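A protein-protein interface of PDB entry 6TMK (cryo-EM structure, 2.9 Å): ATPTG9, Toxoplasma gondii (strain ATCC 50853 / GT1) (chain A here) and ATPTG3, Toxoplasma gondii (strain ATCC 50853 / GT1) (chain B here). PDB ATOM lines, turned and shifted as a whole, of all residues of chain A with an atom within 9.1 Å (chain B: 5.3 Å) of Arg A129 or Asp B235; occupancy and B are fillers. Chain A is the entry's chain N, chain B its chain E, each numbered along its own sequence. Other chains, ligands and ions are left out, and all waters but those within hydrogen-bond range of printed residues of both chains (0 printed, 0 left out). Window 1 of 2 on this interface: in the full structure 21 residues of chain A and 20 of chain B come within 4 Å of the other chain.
NH1 of Arg A129 is in salt-bridge range of OD1 of Asp B201, at 2.7 Å. NH2 of Arg A129 lies within salt-bridge range of OD1 of Asp B233 (3.3 Å). The guanidinium group of Arg A129 is in salt-bridge range of the side-chain carboxylate of Asp B235, at 2.6 Å.
The side-chain amino group of Lys B197 is in salt-bridge range of the side-chain carboxylate of Asp B201, 3.6 Å away. The side-chain amino group of Lys B197 is in salt-bridge range of the side-chain carboxylate of Asp B235 (3.5 Å). N of Asp B235 lies within hydrogen-bond range of OD2 of Asp B233 (3.0 Å).
Among the printed residues, merely in contact across the chains: Ala A126 with Ala B234 (3.8 Å) and Leu A134 with Gly B232 (3.6 Å).
Arg A129 touches three residues of chain B. Of the printed residues of chain A, Asp B235 touches Arg A129 (2.6 Å). Ala B234 touches one residue of chain A. No residue of chain A comes within 4 Å of Ile B236. Printed residues of chain A within 4 Å of Asp B233: Arg A129. Of the printed residues of chain A, Asp B201 touches Arg A129. Of the printed residues of chain B, Leu A134 touches Gly B232. Printed residues of chain A within 4 Å of Gly B232: Leu A134. Ser A130 touches none of the printed residues of chain B. Ser B237 touches none of the printed residues of chain A. The nearest printed residue of chain B that does not touch Ala A126 is Asp B233 (6.1 Å).
Hydrophobic or aromatic side chains of chain B that line the printed part of chain A: Ala B234. Printed residues of chain A that touch a printed residue of chain B: Ala A126, Arg A129 and Leu A134. Among the printed residues, 5 pairs touch across the chains. Among the printed residues, Asp or Glu carboxylates within 4 Å of a Lys or Arg side-chain nitrogen of the other chain: Arg A129 with Asp B201, Arg A129 with Asp B233 and Arg A129 with Asp B235.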
ATOM      1  N   ALA A 126      19.469  17.162  18.113  1.00  0.00           N
ATOM      2  CA  ALA A 126      20.507  17.609  17.211  1.00  0.00           C
ATOM      3  C   ALA A 126      19.904  18.049  15.881  1.00  0.00           C
ATOM      4  O   ALA A 126      18.765  17.707  15.560  1.00  0.00           O
ATOM      5  CB  ALA A 126      21.521  16.498  16.982  1.00  0.00           C
ATOM      6  N   PRO A 127      20.653  18.805  15.085  1.00  0.00           N
ATOM      7  CA  PRO A 127      20.143  19.213  13.776  1.00  0.00           C
ATOM      8  C   PRO A 127      19.992  18.029  12.839  1.00  0.00           C
ATOM      9  O   PRO A 127      20.566  16.956  13.035  1.00  0.00           O
ATOM     10  CB  PRO A 127      21.206  20.187  13.260  1.00  0.00           C
ATOM     11  CG  PRO A 127      22.040  20.529  14.424  1.00  0.00           C
ATOM     12  CD  PRO A 127      21.982  19.371  15.348  1.00  0.00           C
ATOM     13  N   VAL A 128      19.199  18.245  11.804  1.00  0.00           N
ATOM     14  CA  VAL A 128      19.011  17.277  10.735  1.00  0.00           C
ATOM     15  C   VAL A 128      19.959  17.608   9.596  1.00  0.00           C
ATOM     16  O   VAL A 128      20.219  18.783   9.307  1.00  0.00           O
ATOM     17  CB  VAL A 128      17.551  17.262  10.256  1.00  0.00           C
ATOM     18  CG1 VAL A 128      17.350  16.171   9.237  1.00  0.00           C
ATOM     19  CG2 VAL A 128      16.625  17.065  11.433  1.00  0.00           C
ATOM     20  N   ARG A 129      20.478  16.571   8.949  1.00  0.00           N
ATOM     21  CA  ARG A 129      21.461  16.760   7.895  1.00  0.00           C
ATOM     22  C   ARG A 129      20.839  17.511   6.728  1.00  0.00           C
ATOM     23  O   ARG A 129      19.789  17.117   6.212  1.00  0.00           O
ATOM     24  CB  ARG A 129      21.991  15.409   7.426  1.00  0.00           C
ATOM     25  CG  ARG A 129      23.299  15.495   6.668  1.00  0.00           C
ATOM     26  CD  ARG A 129      23.671  14.162   6.054  1.00  0.00           C
ATOM     27  NE  ARG A 129      24.222  13.224   7.025  1.00  0.00           N
ATOM     28  CZ  ARG A 129      25.418  13.355   7.584  1.00  0.00           C
ATOM     29  NH1 ARG A 129      25.850  12.461   8.456  1.00  0.00           N
ATOM     30  NH2 ARG A 129      26.188  14.379   7.269  1.00  0.00           N
ATOM     31  N   SER A 130      21.488  18.592   6.305  1.00  0.00           N
ATOM     32  CA  SER A 130      20.980  19.357   5.176  1.00  0.00           C
ATOM     33  C   SER A 130      22.123  20.059   4.461  1.00  0.00           C
ATOM     34  O   SER A 130      22.910  20.791   5.074  1.00  0.00           O
ATOM     35  CB  SER A 130      19.940  20.382   5.636  1.00  0.00           C
ATOM     36  OG  SER A 130      19.168  20.849   4.545  1.00  0.00           O
ATOM     37  N   LYS A 131      22.184  19.825   3.149  1.00  0.00           N
ATOM     38  CA  LYS A 131      23.095  20.553   2.276  1.00  0.00           C
ATOM     39  C   LYS A 131      22.995  22.054   2.498  1.00  0.00           C
ATOM     40  O   LYS A 131      24.012  22.757   2.528  1.00  0.00           O
ATOM     41  CB  LYS A 131      22.777  20.203   0.826  1.00  0.00           C
ATOM     42  CG  LYS A 131      23.877  20.510  -0.157  1.00  0.00           C
ATOM     43  CD  LYS A 131      23.614  19.827  -1.489  1.00  0.00           C
ATOM     44  CE  LYS A 131      22.401  20.408  -2.191  1.00  0.00           C
ATOM     45  NZ  LYS A 131      22.604  21.845  -2.525  1.00  0.00           N
ATOM     46  N   GLU A 132      21.775  22.563   2.671  1.00  0.00           N
ATOM     47  CA  GLU A 132      21.579  24.002   2.780  1.00  0.00           C
ATOM     48  C   GLU A 132      22.135  24.535   4.092  1.00  0.00           C
ATOM     49  O   GLU A 132      22.774  25.592   4.116  1.00  0.00           O
ATOM     50  CB  GLU A 132      20.096  24.339   2.654  1.00  0.00           C
ATOM     51  CG  GLU A 132      19.497  23.990   1.307  1.00  0.00           C
ATOM     52  CD  GLU A 132      19.072  22.537   1.205  1.00  0.00           C
ATOM     53  OE1 GLU A 132      18.700  22.103   0.095  1.00  0.00           O
ATOM     54  OE2 GLU A 132      19.110  21.826   2.233  1.00  0.00           O
ATOM     55  N   GLN A 133      21.908  23.818   5.191  1.00  0.00           N
ATOM     56  CA  GLN A 133      22.465  24.251   6.467  1.00  0.00           C
ATOM     57  C   GLN A 133      23.985  24.199   6.441  1.00  0.00           C
ATOM     58  O   GLN A 133      24.654  25.096   6.972  1.00  0.00           O
ATOM     59  CB  GLN A 133      21.915  23.392   7.601  1.00  0.00           C
ATOM     60  CG  GLN A 133      20.414  23.485   7.765  1.00  0.00           C
ATOM     61  CD  GLN A 133      19.939  24.898   8.040  1.00  0.00           C
ATOM     62  OE1 GLN A 133      18.974  25.367   7.437  1.00  0.00           O
ATOM     63  NE2 GLN A 133      20.623  25.590   8.940  1.00  0.00           N
ATOM     64  N   LEU A 134      24.553  23.156   5.835  1.00  0.00           N
ATOM     65  CA  LEU A 134      26.005  23.081   5.724  1.00  0.00           C
ATOM     66  C   LEU A 134      26.557  24.251   4.918  1.00  0.00           C
ATOM     67  O   LEU A 134      27.549  24.880   5.308  1.00  0.00           O
ATOM     68  CB  LEU A 134      26.409  21.754   5.090  1.00  0.00           C
ATOM     69  CG  LEU A 134      26.057  20.496   5.877  1.00  0.00           C
ATOM     70  CD1 LEU A 134      26.250  19.274   5.021  1.00  0.00           C
ATOM     71  CD2 LEU A 134      26.892  20.390   7.132  1.00  0.00           C
ATOM     72  N   LYS B 197      30.177   6.762   4.467  1.00  0.00           N
ATOM     73  CA  LYS B 197      29.627   7.313   5.699  1.00  0.00           C
ATOM     74  C   LYS B 197      28.227   7.869   5.479  1.00  0.00           C
ATOM     75  O   LYS B 197      27.352   7.708   6.336  1.00  0.00           O
ATOM     76  CB  LYS B 197      30.565   8.383   6.248  1.00  0.00           C
ATOM     77  CG  LYS B 197      30.005   9.159   7.408  1.00  0.00           C
ATOM     78  CD  LYS B 197      31.097   9.686   8.298  1.00  0.00           C
ATOM     79  CE  LYS B 197      30.576  10.776   9.205  1.00  0.00           C
ATOM     80  NZ  LYS B 197      29.539  10.260  10.125  1.00  0.00           N
ATOM     81  N   ILE B 198      27.987   8.508   4.335  1.00  0.00           N
ATOM     82  CA  ILE B 198      26.671   9.082   4.075  1.00  0.00           C
ATOM     83  C   ILE B 198      25.635   7.975   3.929  1.00  0.00           C
ATOM     84  O   ILE B 198      24.540   8.035   4.506  1.00  0.00           O
ATOM     85  CB  ILE B 198      26.719   9.963   2.814  1.00  0.00           C
ATOM     86  CG1 ILE B 198      27.897  10.940   2.854  1.00  0.00           C
ATOM     87  CG2 ILE B 198      25.419  10.717   2.646  1.00  0.00           C
ATOM     88  CD1 ILE B 198      27.961  11.810   4.068  1.00  0.00           C
ATOM     89  N   ASP B 201      24.902   6.448   7.260  1.00  0.00           N
ATOM     90  CA  ASP B 201      24.026   7.291   8.062  1.00  0.00           C
ATOM     91  C   ASP B 201      22.578   7.144   7.618  1.00  0.00           C
ATOM     92  O   ASP B 201      21.670   7.007   8.447  1.00  0.00           O
ATOM     93  CB  ASP B 201      24.474   8.744   7.958  1.00  0.00           C
ATOM     94  CG  ASP B 201      25.795   9.002   8.659  1.00  0.00           C
ATOM     95  OD1 ASP B 201      26.563   9.861   8.180  1.00  0.00           O
ATOM     96  OD2 ASP B 201      26.065   8.347   9.686  1.00  0.00           O
ATOM     97  N   GLY B 232      26.102  22.908  12.034  1.00  0.00           N
ATOM     98  CA  GLY B 232      25.304  22.521  10.892  1.00  0.00           C
ATOM     99  C   GLY B 232      25.046  21.042  10.744  1.00  0.00           C
ATOM    100  O   GLY B 232      24.415  20.639   9.762  1.00  0.00           O
ATOM    101  N   ASP B 233      25.501  20.218  11.680  1.00  0.00           N
ATOM    102  CA  ASP B 233      25.374  18.777  11.548  1.00  0.00           C
ATOM    103  C   ASP B 233      25.678  18.148  12.895  1.00  0.00           C
ATOM    104  O   ASP B 233      26.473  18.676  13.676  1.00  0.00           O
ATOM    105  CB  ASP B 233      26.318  18.230  10.474  1.00  0.00           C
ATOM    106  CG  ASP B 233      25.964  16.828  10.043  1.00  0.00           C
ATOM    107  OD1 ASP B 233      24.953  16.661   9.332  1.00  0.00           O
ATOM    108  OD2 ASP B 233      26.701  15.894  10.408  1.00  0.00           O
ATOM    109  N   ALA B 234      25.030  17.015  13.158  1.00  0.00           N
ATOM    110  CA  ALA B 234      25.240  16.301  14.406  1.00  0.00           C
ATOM    111  C   ALA B 234      26.616  15.659  14.478  1.00  0.00           C
ATOM    112  O   ALA B 234      27.079  15.335  15.575  1.00  0.00           O
ATOM    113  CB  ALA B 234      24.158  15.242  14.582  1.00  0.00           C
ATOM    114  N   ASP B 235      27.273  15.470  13.339  1.00  0.00           N
ATOM    115  CA  ASP B 235      28.612  14.905  13.326  1.00  0.00           C
ATOM    116  C   ASP B 235      29.676  15.899  13.766  1.00  0.00           C
ATOM    117  O   ASP B 235      30.769  15.478  14.156  1.00  0.00           O
ATOM    118  CB  ASP B 235      28.938  14.370  11.931  1.00  0.00           C
ATOM    119  CG  ASP B 235      27.937  13.336  11.456  1.00  0.00           C
ATOM    120  OD1 ASP B 235      27.417  13.483  10.330  1.00  0.00           O
ATOM    121  OD2 ASP B 235      27.664  12.380  12.211  1.00  0.00           O
ATOM    122  N   ILE B 236      29.390  17.197  13.720  1.00  0.00           N
ATOM    123  CA  ILE B 236      30.373  18.233  14.007  1.00  0.00           C
ATOM    124  C   ILE B 236      29.850  19.021  15.198  1.00  0.00           C
ATOM    125  O   ILE B 236      28.936  19.844  15.063  1.00  0.00           O
ATOM    126  CB  ILE B 236      30.624  19.148  12.806  1.00  0.00           C
ATOM    127  CG1 ILE B 236      31.001  18.333  11.575  1.00  0.00           C
ATOM    128  CG2 ILE B 236      31.731  20.127  13.121  1.00  0.00           C
ATOM    129  CD1 ILE B 236      30.737  19.051  10.294  1.00  0.00           C
ATOM    130  N   SER B 237      30.433  18.780  16.368  1.00  0.00           N
ATOM    131  CA  SER B 237      30.004  19.418  17.597  1.00  0.00           C
ATOM    132  C   SER B 237      31.210  19.688  18.482  1.00  0.00           C
ATOM    133  O   SER B 237      32.271  19.079  18.331  1.00  0.00           O
ATOM    134  CB  SER B 237      28.995  18.550  18.348  1.00  0.00           C
ATOM    135  OG  SER B 237      29.572  17.315  18.722  1.00  0.00           O
